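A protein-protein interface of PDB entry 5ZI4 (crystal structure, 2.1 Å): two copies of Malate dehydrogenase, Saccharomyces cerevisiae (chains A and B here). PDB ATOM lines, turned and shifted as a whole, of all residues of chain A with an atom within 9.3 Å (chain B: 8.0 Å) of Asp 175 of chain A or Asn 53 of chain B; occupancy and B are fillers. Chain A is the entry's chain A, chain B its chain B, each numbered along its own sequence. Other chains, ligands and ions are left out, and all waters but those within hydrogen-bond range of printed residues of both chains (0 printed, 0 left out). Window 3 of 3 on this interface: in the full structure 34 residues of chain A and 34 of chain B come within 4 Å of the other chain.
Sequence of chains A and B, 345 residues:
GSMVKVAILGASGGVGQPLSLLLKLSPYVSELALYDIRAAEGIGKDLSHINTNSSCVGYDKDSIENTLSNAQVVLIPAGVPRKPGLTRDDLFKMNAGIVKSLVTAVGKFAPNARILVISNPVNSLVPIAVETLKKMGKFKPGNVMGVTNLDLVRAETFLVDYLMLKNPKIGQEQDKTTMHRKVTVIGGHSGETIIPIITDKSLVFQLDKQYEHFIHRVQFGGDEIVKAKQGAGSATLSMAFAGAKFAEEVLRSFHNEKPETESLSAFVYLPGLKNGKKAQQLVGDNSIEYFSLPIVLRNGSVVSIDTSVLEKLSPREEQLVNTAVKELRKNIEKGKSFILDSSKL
Among the printed residues, pairs that only touch across the chains: Thr 177 of chain A with Asn 51 of chain B, Phe 241 of chain A with Asn 51 of chain B, Lys 176 of chain A with Thr 52 of chain B, Phe 241 of chain A with Leu 25 of chain B, Phe 241 of chain A with Ile 50 of chain B and Thr 177 of chain A with Thr 52 of chain B.
The backbone NH of Asn 51 of chain B sits close to the side-chain hydroxyl of Thr 157 of chain A (3.2 Å). The side-chain carboxylate (OD1) of Asp 175 of chain A is in hydrogen-bond range of the side-chain amide nitrogen (ND2) of Asn 53 of chain B, 2.7 Å away. The side-chain hydroxyl of Thr 157 of chain A sits close to the backbone carbonyl oxygen of Ile 50 of chain B (3.5 Å). OE1 of Glu 156 of chain A sits at hydrogen-bond distance from ND2 of Asn 51 of chain B (3.1 Å). The backbone NH (N) of Lys 176 of chain A sits at hydrogen-bond distance from the side-chain amide oxygen (OD1) of Asn 53 of chain B (3.1 Å). The side-chain amide nitrogen (ND2) of Asn 51 of chain B lies within hydrogen-bond range of the backbone carbonyl oxygen (O) of Lys 176 of chain A (3.1 Å).
No position is printed for both chains.
N of Met 179 of chain A lies within hydrogen-bond range of OE1 of Glu 156 of chain A. OG1 of Thr 177 of chain A is in hydrogen-bond range of OD1 of Asp 175 of chain A, at 2.4 Å. The backbone NH (N) of His 180 of chain A is in hydrogen-bond range of the side-chain carboxylate (OE1) of Glu 156 of chain A (2.9 Å). NZ of Lys 24 of chain B sits at hydrogen-bond distance from OG1 of Thr 52 of chain B (2.6 Å). The side-chain carboxylate (OD1) of Asp 161 of chain A is in salt-bridge range of the side-chain amino group (NZ) of Lys 176 of chain A, 2.7 Å away. O of Ile 50 of chain B is in hydrogen-bond range of NZ of Lys 24 of chain B (3.4 Å).
Of the 14 printed residues of chain B, 5 touch a printed residue of chain A. Printed residues of chain A that touch a printed residue of chain B: Glu 156, Thr 157, Asp 175, Lys 176, Thr 177 and Phe 241. Hydrophobic or aromatic side chains of chain A that line the printed part of chain B: Phe 241. Among the printed residues, 12 pairs touch across the chains. Among the printed residues, no Asp or Glu carboxylate lies within 4 Å of a Lys or Arg side-chain nitrogen of the other chain.
Printed residues of chain B within 4 Å of Glu 156 of chain A: Asn 51. Asp 175 of chain A touches one residue of chain B. Lys 182 of chain A touches none of the printed residues of chain B. Val 183 of chain A touches none of the printed residues of chain B. Of the printed residues of chain A, Leu 25 of chain B touches Phe 241. Printed residues of chain A within 4 Å of Asn 53 of chain B: Asp 175 (2.7 Å) and Lys 176 (3.1 Å). No residue of chain A comes within 4 Å of Ser 54 of chain B. The nearest residue of chain B that does not touch Asp 175 of chain A is Asn 51 of chain B (6.1 Å). The nearest printed residue of chain B that does not touch Phe 241 of chain A is Thr 52 of chain B (5.0 Å).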
ATOM      1  N   GLU A 156      -9.783  -3.765 -28.055  1.00  0.00           N
ATOM      2  CA  GLU A 156     -10.003  -3.008 -26.833  1.00  0.00           C
ATOM      3  C   GLU A 156      -9.835  -1.495 -27.015  1.00  0.00           C
ATOM      4  O   GLU A 156     -10.697  -0.714 -26.626  1.00  0.00           O
ATOM      5  CB  GLU A 156      -9.041  -3.502 -25.755  1.00  0.00           C
ATOM      6  CG  GLU A 156      -9.553  -4.768 -25.131  1.00  0.00           C
ATOM      7  CD  GLU A 156      -8.615  -5.427 -24.147  1.00  0.00           C
ATOM      8  OE1 GLU A 156      -8.731  -5.245 -22.916  1.00  0.00           O
ATOM      9  OE2 GLU A 156      -7.747  -6.166 -24.613  1.00  0.00           O
ATOM     10  N   THR A 157      -8.725  -1.105 -27.624  1.00  0.00           N
ATOM     11  CA  THR A 157      -8.402   0.285 -27.807  1.00  0.00           C
ATOM     12  C   THR A 157      -9.269   0.979 -28.905  1.00  0.00           C
ATOM     13  O   THR A 157      -9.765   2.117 -28.698  1.00  0.00           O
ATOM     14  CB  THR A 157      -6.869   0.440 -28.120  1.00  0.00           C
ATOM     15  OG1 THR A 157      -6.088  -0.051 -27.019  1.00  0.00           O
ATOM     16  CG2 THR A 157      -6.475   1.884 -28.391  1.00  0.00           C
ATOM     17  N   LEU A 159     -12.136   0.086 -29.853  1.00  0.00           N
ATOM     18  CA  LEU A 159     -13.533  -0.028 -29.449  1.00  0.00           C
ATOM     19  C   LEU A 159     -13.847   1.295 -28.773  1.00  0.00           C
ATOM     20  O   LEU A 159     -14.712   2.057 -29.274  1.00  0.00           O
ATOM     21  CB  LEU A 159     -13.813  -1.251 -28.536  1.00  0.00           C
ATOM     22  CG  LEU A 159     -15.299  -1.542 -28.185  1.00  0.00           C
ATOM     23  CD1 LEU A 159     -16.283  -1.307 -29.347  1.00  0.00           C
ATOM     24  CD2 LEU A 159     -15.468  -2.964 -27.659  1.00  0.00           C
ATOM     25  N   VAL A 160     -13.053   1.613 -27.742  1.00  0.00           N
ATOM     26  CA  VAL A 160     -13.136   2.934 -27.091  1.00  0.00           C
ATOM     27  C   VAL A 160     -12.883   4.121 -28.061  1.00  0.00           C
ATOM     28  O   VAL A 160     -13.766   4.973 -28.262  1.00  0.00           O
ATOM     29  CB  VAL A 160     -12.296   3.008 -25.840  1.00  0.00           C
ATOM     30  CG1 VAL A 160     -12.652   4.276 -25.089  1.00  0.00           C
ATOM     31  CG2 VAL A 160     -12.538   1.786 -24.939  1.00  0.00           C
ATOM     32  N   ASP A 161     -11.747   4.206 -28.726  1.00  0.00           N
ATOM     33  CA  ASP A 161     -11.641   5.313 -29.688  1.00  0.00           C
ATOM     34  C   ASP A 161     -12.945   5.540 -30.535  1.00  0.00           C
ATOM     35  O   ASP A 161     -13.384   6.693 -30.733  1.00  0.00           O
ATOM     36  CB  ASP A 161     -10.488   5.141 -30.657  1.00  0.00           C
ATOM     37  CG  ASP A 161      -9.150   4.985 -29.976  1.00  0.00           C
ATOM     38  OD1 ASP A 161      -9.064   5.075 -28.709  1.00  0.00           O
ATOM     39  OD2 ASP A 161      -8.214   4.736 -30.777  1.00  0.00           O
ATOM     40  N   LEU A 163     -16.142   4.469 -29.954  1.00  0.00           N
ATOM     41  CA  LEU A 163     -17.255   4.841 -29.069  1.00  0.00           C
ATOM     42  C   LEU A 163     -17.239   6.351 -28.789  1.00  0.00           C
ATOM     43  O   LEU A 163     -18.241   7.045 -29.026  1.00  0.00           O
ATOM     44  CB  LEU A 163     -17.252   4.039 -27.732  1.00  0.00           C
ATOM     45  CG  LEU A 163     -17.640   2.543 -27.703  1.00  0.00           C
ATOM     46  CD1 LEU A 163     -18.127   2.139 -26.315  1.00  0.00           C
ATOM     47  CD2 LEU A 163     -18.673   2.167 -28.761  1.00  0.00           C
ATOM     48  N   MET A 164     -16.082   6.854 -28.357  1.00  0.00           N
ATOM     49  CA  MET A 164     -15.888   8.276 -28.081  1.00  0.00           C
ATOM     50  C   MET A 164     -16.471   9.169 -29.150  1.00  0.00           C
ATOM     51  O   MET A 164     -17.229  10.096 -28.850  1.00  0.00           O
ATOM     52  CB  MET A 164     -14.399   8.597 -27.966  1.00  0.00           C
ATOM     53  CG  MET A 164     -13.769   8.097 -26.709  1.00  0.00           C
ATOM     54  SD  MET A 164     -14.492   8.932 -25.305  1.00  0.00           S
ATOM     55  CE  MET A 164     -13.230   8.399 -24.130  1.00  0.00           C
ATOM     56  N   ILE A 170     -20.831   7.454 -23.215  1.00  0.00           N
ATOM     57  CA  ILE A 170     -20.417   6.035 -23.047  1.00  0.00           C
ATOM     58  C   ILE A 170     -18.918   5.798 -23.290  1.00  0.00           C
ATOM     59  O   ILE A 170     -18.285   5.095 -22.491  1.00  0.00           O
ATOM     60  CB  ILE A 170     -21.313   5.005 -23.822  1.00  0.00           C
ATOM     61  CG1 ILE A 170     -21.158   3.590 -23.235  1.00  0.00           C
ATOM     62  CG2 ILE A 170     -21.014   4.966 -25.320  1.00  0.00           C
ATOM     63  CD1 ILE A 170     -22.216   2.604 -23.680  1.00  0.00           C
ATOM     64  N   GLY A 171     -18.346   6.414 -24.333  1.00  0.00           N
ATOM     65  CA  GLY A 171     -16.892   6.360 -24.579  1.00  0.00           C
ATOM     66  C   GLY A 171     -16.090   6.544 -23.289  1.00  0.00           C
ATOM     67  O   GLY A 171     -15.270   5.689 -22.910  1.00  0.00           O
ATOM     68  N   GLN A 172     -16.397   7.641 -22.591  1.00  0.00           N
ATOM     69  CA  GLN A 172     -15.761   8.023 -21.315  1.00  0.00           C
ATOM     70  C   GLN A 172     -16.050   7.060 -20.166  1.00  0.00           C
ATOM     71  O   GLN A 172     -15.298   7.014 -19.202  1.00  0.00           O
ATOM     72  CB  GLN A 172     -16.171   9.459 -20.917  1.00  0.00           C
ATOM     73  CG  GLN A 172     -15.705  10.563 -21.889  1.00  0.00           C
ATOM     74  CD  GLN A 172     -14.201  10.886 -21.845  1.00  0.00           C
ATOM     75  OE1 GLN A 172     -13.622  11.264 -22.867  1.00  0.00           O
ATOM     76  NE2 GLN A 172     -13.566  10.750 -20.667  1.00  0.00           N
ATOM     77  N   GLU A 173     -17.127   6.289 -20.264  1.00  0.00           N
ATOM     78  CA  GLU A 173     -17.469   5.300 -19.233  1.00  0.00           C
ATOM     79  C   GLU A 173     -16.561   4.058 -19.230  1.00  0.00           C
ATOM     80  O   GLU A 173     -16.541   3.281 -18.260  1.00  0.00           O
ATOM     81  CB  GLU A 173     -18.937   4.894 -19.387  1.00  0.00           C
ATOM     82  CG  GLU A 173     -19.912   5.997 -18.968  1.00  0.00           C
ATOM     83  CD  GLU A 173     -21.267   5.948 -19.668  1.00  0.00           C
ATOM     84  OE1 GLU A 173     -22.013   6.942 -19.543  1.00  0.00           O
ATOM     85  OE2 GLU A 173     -21.596   4.947 -20.344  1.00  0.00           O
ATOM     86  N   GLN A 174     -15.799   3.884 -20.311  1.00  0.00           N
ATOM     87  CA  GLN A 174     -15.008   2.672 -20.498  1.00  0.00           C
ATOM     88  C   GLN A 174     -13.574   2.779 -19.972  1.00  0.00           C
ATOM     89  O   GLN A 174     -12.940   3.852 -19.965  1.00  0.00           O
ATOM     90  CB  GLN A 174     -14.979   2.295 -21.972  1.00  0.00           C
ATOM     91  CG  GLN A 174     -16.346   2.184 -22.629  1.00  0.00           C
ATOM     92  CD  GLN A 174     -17.252   1.125 -22.013  1.00  0.00           C
ATOM     93  OE1 GLN A 174     -16.850   0.328 -21.141  1.00  0.00           O
ATOM     94  NE2 GLN A 174     -18.492   1.101 -22.492  1.00  0.00           N
ATOM     95  N   ASP A 175     -13.078   1.645 -19.517  1.00  0.00           N
ATOM     96  CA  ASP A 175     -11.711   1.532 -19.108  1.00  0.00           C
ATOM     97  C   ASP A 175     -11.016   0.711 -20.232  1.00  0.00           C
ATOM     98  O   ASP A 175     -11.191  -0.519 -20.282  1.00  0.00           O
ATOM     99  CB  ASP A 175     -11.686   0.881 -17.737  1.00  0.00           C
ATOM    100  CG  ASP A 175     -10.339   0.814 -17.171  1.00  0.00           C
ATOM    101  OD1 ASP A 175      -9.409   1.078 -17.948  1.00  0.00           O
ATOM    102  OD2 ASP A 175     -10.192   0.464 -15.969  1.00  0.00           O
ATOM    103  N   LYS A 176     -10.289   1.402 -21.149  1.00  0.00           N
ATOM    104  CA  LYS A 176      -9.473   0.742 -22.211  1.00  0.00           C
ATOM    105  C   LYS A 176      -8.764  -0.501 -21.691  1.00  0.00           C
ATOM    106  O   LYS A 176      -8.713  -1.523 -22.397  1.00  0.00           O
ATOM    107  CB  LYS A 176      -8.426   1.664 -22.851  1.00  0.00           C
ATOM    108  CG  LYS A 176      -8.930   2.476 -24.027  1.00  0.00           C
ATOM    109  CD  LYS A 176      -7.801   3.005 -24.896  1.00  0.00           C
ATOM    110  CE  LYS A 176      -7.729   4.494 -24.985  1.00  0.00           C
ATOM    111  NZ  LYS A 176      -7.709   4.891 -26.425  1.00  0.00           N
ATOM    112  N   THR A 177      -8.300  -0.470 -20.434  1.00  0.00           N
ATOM    113  CA  THR A 177      -7.566  -1.622 -19.885  1.00  0.00           C
ATOM    114  C   THR A 177      -8.319  -2.919 -19.569  1.00  0.00           C
ATOM    115  O   THR A 177      -7.675  -3.968 -19.526  1.00  0.00           O
ATOM    116  CB  THR A 177      -6.877  -1.233 -18.589  1.00  0.00           C
ATOM    117  OG1 THR A 177      -7.890  -0.814 -17.652  1.00  0.00           O
ATOM    118  CG2 THR A 177      -5.843  -0.050 -18.838  1.00  0.00           C
ATOM    119  N   THR A 178      -9.620  -2.872 -19.251  1.00  0.00           N
ATOM    120  CA  THR A 178     -10.346  -4.098 -18.822  1.00  0.00           C
ATOM    121  C   THR A 178     -11.351  -4.494 -19.866  1.00  0.00           C
ATOM    122  O   THR A 178     -12.236  -5.301 -19.606  1.00  0.00           O
ATOM    123  CB  THR A 178     -11.124  -3.982 -17.457  1.00  0.00           C
ATOM    124  OG1 THR A 178     -12.097  -2.946 -17.547  1.00  0.00           O
ATOM    125  CG2 THR A 178     -10.247  -3.732 -16.311  1.00  0.00           C
ATOM    126  N   MET A 179     -11.177  -3.997 -21.081  1.00  0.00           N
ATOM    127  CA  MET A 179     -12.159  -4.219 -22.106  1.00  0.00           C
ATOM    128  C   MET A 179     -12.101  -5.545 -22.903  1.00  0.00           C
ATOM    129  O   MET A 179     -12.814  -5.743 -23.909  1.00  0.00           O
ATOM    130  CB  MET A 179     -12.287  -2.959 -22.902  1.00  0.00           C
ATOM    131  CG  MET A 179     -13.428  -2.155 -22.247  1.00  0.00           C
ATOM    132  SD  MET A 179     -14.065  -1.105 -23.525  1.00  0.00           S
ATOM    133  CE  MET A 179     -14.932  -2.166 -24.663  1.00  0.00           C
ATOM    134  N   HIS A 180     -11.271  -6.449 -22.394  1.00  0.00           N
ATOM    135  CA  HIS A 180     -11.293  -7.859 -22.726  1.00  0.00           C
ATOM    136  C   HIS A 180     -12.500  -8.644 -22.149  1.00  0.00           C
ATOM    137  O   HIS A 180     -12.524  -9.887 -22.239  1.00  0.00           O
ATOM    138  CB  HIS A 180      -9.984  -8.505 -22.248  1.00  0.00           C
ATOM    139  CG  HIS A 180      -9.665  -8.251 -20.813  1.00  0.00           C
ATOM    140  ND1 HIS A 180     -10.381  -8.815 -19.780  1.00  0.00           N
ATOM    141  CD2 HIS A 180      -8.687  -7.512 -20.237  1.00  0.00           C
ATOM    142  CE1 HIS A 180      -9.859  -8.431 -18.628  1.00  0.00           C
ATOM    143  NE2 HIS A 180      -8.827  -7.645 -18.878  1.00  0.00           N
ATOM    144  N   ARG A 181     -13.442  -7.957 -21.490  1.00  0.00           N
ATOM    145  CA  ARG A 181     -14.710  -8.593 -21.095  1.00  0.00           C
ATOM    146  C   ARG A 181     -15.781  -8.248 -22.104  1.00  0.00           C
ATOM    147  O   ARG A 181     -16.781  -8.941 -22.199  1.00  0.00           O
ATOM    148  CB  ARG A 181     -15.090  -8.203 -19.676  1.00  0.00           C
ATOM    149  CG  ARG A 181     -13.959  -8.491 -18.703  1.00  0.00           C
ATOM    150  CD  ARG A 181     -14.422  -8.576 -17.265  1.00  0.00           C
ATOM    151  NE  ARG A 181     -13.368  -8.143 -16.339  1.00  0.00           N
ATOM    152  CZ  ARG A 181     -13.111  -6.874 -15.994  1.00  0.00           C
ATOM    153  NH1 ARG A 181     -13.820  -5.858 -16.495  1.00  0.00           N
ATOM    154  NH2 ARG A 181     -12.123  -6.606 -15.140  1.00  0.00           N
ATOM    155  N   LYS A 182     -15.529  -7.223 -22.905  1.00  0.00           N
ATOM    156  CA  LYS A 182     -16.458  -6.762 -23.904  1.00  0.00           C
ATOM    157  C   LYS A 182     -15.987  -6.943 -25.365  1.00  0.00           C
ATOM    158  O   LYS A 182     -16.735  -6.597 -26.306  1.00  0.00           O
ATOM    159  CB  LYS A 182     -16.747  -5.268 -23.675  1.00  0.00           C
ATOM    160  CG  LYS A 182     -17.259  -4.865 -22.291  1.00  0.00           C
ATOM    161  CD  LYS A 182     -18.089  -3.579 -22.412  1.00  0.00           C
ATOM    162  CE  LYS A 182     -18.578  -3.018 -21.085  1.00  0.00           C
ATOM    163  NZ  LYS A 182     -17.503  -2.312 -20.343  1.00  0.00           N
ATOM    164  N   VAL A 183     -14.764  -7.423 -25.592  1.00  0.00           N
ATOM    165  CA  VAL A 183     -14.363  -7.754 -26.969  1.00  0.00           C
ATOM    166  C   VAL A 183     -13.341  -8.872 -26.875  1.00  0.00           C
ATOM    167  O   VAL A 183     -12.608  -8.988 -25.890  1.00  0.00           O
ATOM    168  CB  VAL A 183     -13.954  -6.510 -27.816  1.00  0.00           C
ATOM    169  CG1 VAL A 183     -12.757  -5.773 -27.221  1.00  0.00           C
ATOM    170  CG2 VAL A 183     -13.739  -6.866 -29.291  1.00  0.00           C
ATOM    171  N   PHE A 241       4.557  -4.854 -25.584  1.00  0.00           N
ATOM    172  CA  PHE A 241       3.519  -4.794 -24.579  1.00  0.00           C
ATOM    173  C   PHE A 241       2.580  -5.995 -24.655  1.00  0.00           C
ATOM    174  O   PHE A 241       2.482  -6.713 -23.697  1.00  0.00           O
ATOM    175  CB  PHE A 241       2.734  -3.497 -24.709  1.00  0.00           C
ATOM    176  CG  PHE A 241       1.513  -3.450 -23.837  1.00  0.00           C
ATOM    177  CD1 PHE A 241       1.617  -3.209 -22.486  1.00  0.00           C
ATOM    178  CD2 PHE A 241       0.255  -3.686 -24.383  1.00  0.00           C
ATOM    179  CE1 PHE A 241       0.492  -3.184 -21.698  1.00  0.00           C
ATOM    180  CE2 PHE A 241      -0.881  -3.648 -23.587  1.00  0.00           C
ATOM    181  CZ  PHE A 241      -0.758  -3.407 -22.247  1.00  0.00           C
ATOM    182  N   GLU A 260      -5.614 -12.871 -15.726  1.00  0.00           N
ATOM    183  CA  GLU A 260      -6.191 -11.546 -15.619  1.00  0.00           C
ATOM    184  C   GLU A 260      -7.046 -11.222 -16.856  1.00  0.00           C
ATOM    185  O   GLU A 260      -7.991 -10.431 -16.754  1.00  0.00           O
ATOM    186  CB  GLU A 260      -5.065 -10.509 -15.398  1.00  0.00           C
ATOM    187  CG  GLU A 260      -5.503  -9.068 -15.072  1.00  0.00           C
ATOM    188  CD  GLU A 260      -5.444  -8.078 -16.254  1.00  0.00           C
ATOM    189  OE1 GLU A 260      -6.365  -7.228 -16.362  1.00  0.00           O
ATOM    190  OE2 GLU A 260      -4.482  -8.116 -17.061  1.00  0.00           O
ATOM    191  N   LYS B  24       3.444   5.301 -21.405  1.00  0.00           N
ATOM    192  CA  LYS B  24       2.106   4.983 -21.931  1.00  0.00           C
ATOM    193  C   LYS B  24       1.399   4.064 -20.982  1.00  0.00           C
ATOM    194  O   LYS B  24       0.196   4.145 -20.900  1.00  0.00           O
ATOM    195  CB  LYS B  24       2.108   4.409 -23.373  1.00  0.00           C
ATOM    196  CG  LYS B  24       0.715   4.058 -23.949  1.00  0.00           C
ATOM    197  CD  LYS B  24       0.011   5.219 -24.627  1.00  0.00           C
ATOM    198  CE  LYS B  24      -1.417   4.911 -25.096  1.00  0.00           C
ATOM    199  NZ  LYS B  24      -2.228   4.423 -23.950  1.00  0.00           N
ATOM    200  N   LEU B  25       2.144   3.251 -20.228  1.00  0.00           N
ATOM    201  CA  LEU B  25       1.579   2.364 -19.218  1.00  0.00           C
ATOM    202  C   LEU B  25       1.246   3.002 -17.860  1.00  0.00           C
ATOM    203  O   LEU B  25       0.747   2.314 -16.962  1.00  0.00           O
ATOM    204  CB  LEU B  25       2.557   1.219 -18.915  1.00  0.00           C
ATOM    205  CG  LEU B  25       3.120   0.420 -20.074  1.00  0.00           C
ATOM    206  CD1 LEU B  25       3.906  -0.732 -19.502  1.00  0.00           C
ATOM    207  CD2 LEU B  25       2.033  -0.036 -20.996  1.00  0.00           C
ATOM    208  N   SER B  26       1.530   4.282 -17.683  1.00  0.00           N
ATOM    209  CA  SER B  26       1.285   4.928 -16.414  1.00  0.00           C
ATOM    210  C   SER B  26      -0.179   5.313 -16.261  1.00  0.00           C
ATOM    211  O   SER B  26      -0.679   6.021 -17.110  1.00  0.00           O
ATOM    212  CB  SER B  26       2.132   6.218 -16.341  1.00  0.00           C
ATOM    213  OG  SER B  26       1.898   6.903 -15.129  1.00  0.00           O
ATOM    214  N   PRO B  27      -0.832   4.945 -15.140  1.00  0.00           N
ATOM    215  CA  PRO B  27      -2.223   5.443 -14.911  1.00  0.00           C
ATOM    216  C   PRO B  27      -2.343   6.937 -14.577  1.00  0.00           C
ATOM    217  O   PRO B  27      -3.419   7.472 -14.601  1.00  0.00           O
ATOM    218  CB  PRO B  27      -2.686   4.611 -13.743  1.00  0.00           C
ATOM    219  CG  PRO B  27      -1.451   4.393 -12.948  1.00  0.00           C
ATOM    220  CD  PRO B  27      -0.334   4.211 -13.961  1.00  0.00           C
ATOM    221  N   VAL B  29      -1.125   9.509 -16.314  1.00  0.00           N
ATOM    222  CA  VAL B  29      -0.929  10.307 -17.475  1.00  0.00           C
ATOM    223  C   VAL B  29      -2.213  10.300 -18.270  1.00  0.00           C
ATOM    224  O   VAL B  29      -2.812   9.241 -18.484  1.00  0.00           O
ATOM    225  CB  VAL B  29       0.176   9.709 -18.363  1.00  0.00           C
ATOM    226  CG1 VAL B  29       0.355  10.562 -19.616  1.00  0.00           C
ATOM    227  CG2 VAL B  29       1.477   9.562 -17.586  1.00  0.00           C
ATOM    228  N   SER B  30      -2.555  11.468 -18.794  1.00  0.00           N
ATOM    229  CA  SER B  30      -3.763  11.643 -19.505  1.00  0.00           C
ATOM    230  C   SER B  30      -3.475  11.904 -20.984  1.00  0.00           C
ATOM    231  O   SER B  30      -4.142  11.335 -21.839  1.00  0.00           O
ATOM    232  CB  SER B  30      -4.537  12.780 -18.828  1.00  0.00           C
ATOM    233  OG  SER B  30      -4.712  12.456 -17.415  1.00  0.00           O
ATOM    234  N   GLU B  31      -2.516  12.770 -21.281  1.00  0.00           N
ATOM    235  CA  GLU B  31      -1.944  12.845 -22.637  1.00  0.00           C
ATOM    236  C   GLU B  31      -0.453  12.624 -22.537  1.00  0.00           C
ATOM    237  O   GLU B  31       0.209  12.991 -21.507  1.00  0.00           O
ATOM    238  CB  GLU B  31      -2.195  14.181 -23.324  1.00  0.00           C
ATOM    239  CG  GLU B  31      -3.658  14.485 -23.566  1.00  0.00           C
ATOM    240  CD  GLU B  31      -3.966  15.892 -23.184  1.00  0.00           C
ATOM    241  OE1 GLU B  31      -4.665  16.040 -22.186  1.00  0.00           O
ATOM    242  OE2 GLU B  31      -3.429  16.825 -23.826  1.00  0.00           O
ATOM    243  N   ILE B  50      -1.836   0.770 -27.705  1.00  0.00           N
ATOM    244  CA  ILE B  50      -1.825   0.088 -26.402  1.00  0.00           C
ATOM    245  C   ILE B  50      -3.086   0.456 -25.592  1.00  0.00           C
ATOM    246  O   ILE B  50      -3.437   1.616 -25.472  1.00  0.00           O
ATOM    247  CB  ILE B  50      -0.571   0.423 -25.576  1.00  0.00           C
ATOM    248  CG1 ILE B  50       0.700  -0.157 -26.206  1.00  0.00           C
ATOM    249  CG2 ILE B  50      -0.683  -0.084 -24.178  1.00  0.00           C
ATOM    250  CD1 ILE B  50       1.972   0.187 -25.450  1.00  0.00           C
ATOM    251  N   ASN B  51      -3.705  -0.536 -24.976  1.00  0.00           N
ATOM    252  CA  ASN B  51      -5.001  -0.368 -24.304  1.00  0.00           C
ATOM    253  C   ASN B  51      -4.821   0.162 -22.874  1.00  0.00           C
ATOM    254  O   ASN B  51      -5.116  -0.518 -21.914  1.00  0.00           O
ATOM    255  CB  ASN B  51      -5.850  -1.663 -24.366  1.00  0.00           C
ATOM    256  CG  ASN B  51      -5.328  -2.790 -23.467  1.00  0.00           C
ATOM    257  OD1 ASN B  51      -4.145  -3.115 -23.460  1.00  0.00           O
ATOM    258  ND2 ASN B  51      -6.221  -3.406 -22.717  1.00  0.00           N
ATOM    259  N   THR B  52      -4.260   1.370 -22.777  1.00  0.00           N
ATOM    260  CA  THR B  52      -4.208   2.139 -21.528  1.00  0.00           C
ATOM    261  C   THR B  52      -4.767   3.509 -21.822  1.00  0.00           C
ATOM    262  O   THR B  52      -4.885   3.978 -22.985  1.00  0.00           O
ATOM    263  CB  THR B  52      -2.795   2.279 -20.928  1.00  0.00           C
ATOM    264  OG1 THR B  52      -1.942   2.833 -21.917  1.00  0.00           O
ATOM    265  CG2 THR B  52      -2.279   0.985 -20.468  1.00  0.00           C
ATOM    266  N   ASN B  53      -5.141   4.176 -20.757  1.00  0.00           N
ATOM    267  CA  ASN B  53      -6.108   5.242 -20.870  1.00  0.00           C
ATOM    268  C   ASN B  53      -5.591   6.542 -21.497  1.00  0.00           C
ATOM    269  O   ASN B  53      -6.348   7.281 -22.097  1.00  0.00           O
ATOM    270  CB  ASN B  53      -6.943   5.289 -19.549  1.00  0.00           C
ATOM    271  CG  ASN B  53      -7.998   4.152 -19.520  1.00  0.00           C
ATOM    272  OD1 ASN B  53      -8.748   3.982 -20.486  1.00  0.00           O
ATOM    273  ND2 ASN B  53      -8.055   3.393 -18.465  1.00  0.00           N
ATOM    274  N   SER B  54      -4.284   6.686 -21.606  1.00  0.00           N
ATOM    275  CA  SER B  54      -3.695   7.885 -22.119  1.00  0.00           C
ATOM    276  C   SER B  54      -3.823   8.059 -23.658  1.00  0.00           C
ATOM    277  O   SER B  54      -3.814   7.098 -24.426  1.00  0.00           O
ATOM    278  CB  SER B  54      -2.229   7.898 -21.657  1.00  0.00           C
ATOM    279  OG  SER B  54      -1.559   6.671 -21.907  1.00  0.00           O
ATOM    280  N   SER B  55      -3.998   9.282 -24.103  1.00  0.00           N
ATOM    281  CA  SER B  55      -3.853   9.582 -25.517  1.00  0.00           C
ATOM    282  C   SER B  55      -2.378   9.762 -25.744  1.00  0.00           C
ATOM    283  O   SER B  55      -1.667  10.288 -24.871  1.00  0.00           O
ATOM    284  CB  SER B  55      -4.571  10.862 -25.853  1.00  0.00           C
ATOM    285  OG  SER B  55      -5.680  10.892 -25.027  1.00  0.00           O
ATOM    286  N   CYS B  56      -1.916   9.321 -26.903  1.00  0.00           N
ATOM    287  CA  CYS B  56      -0.529   9.352 -27.243  1.00  0.00           C
ATOM    288  C   CYS B  56      -0.441   9.818 -28.656  1.00  0.00           C
ATOM    289  O   CYS B  56      -0.951   9.160 -29.566  1.00  0.00           O
ATOM    290  CB  CYS B  56       0.113   7.985 -27.086  1.00  0.00           C
ATOM    291  SG  CYS B  56       1.904   8.090 -27.334  1.00  0.00           S
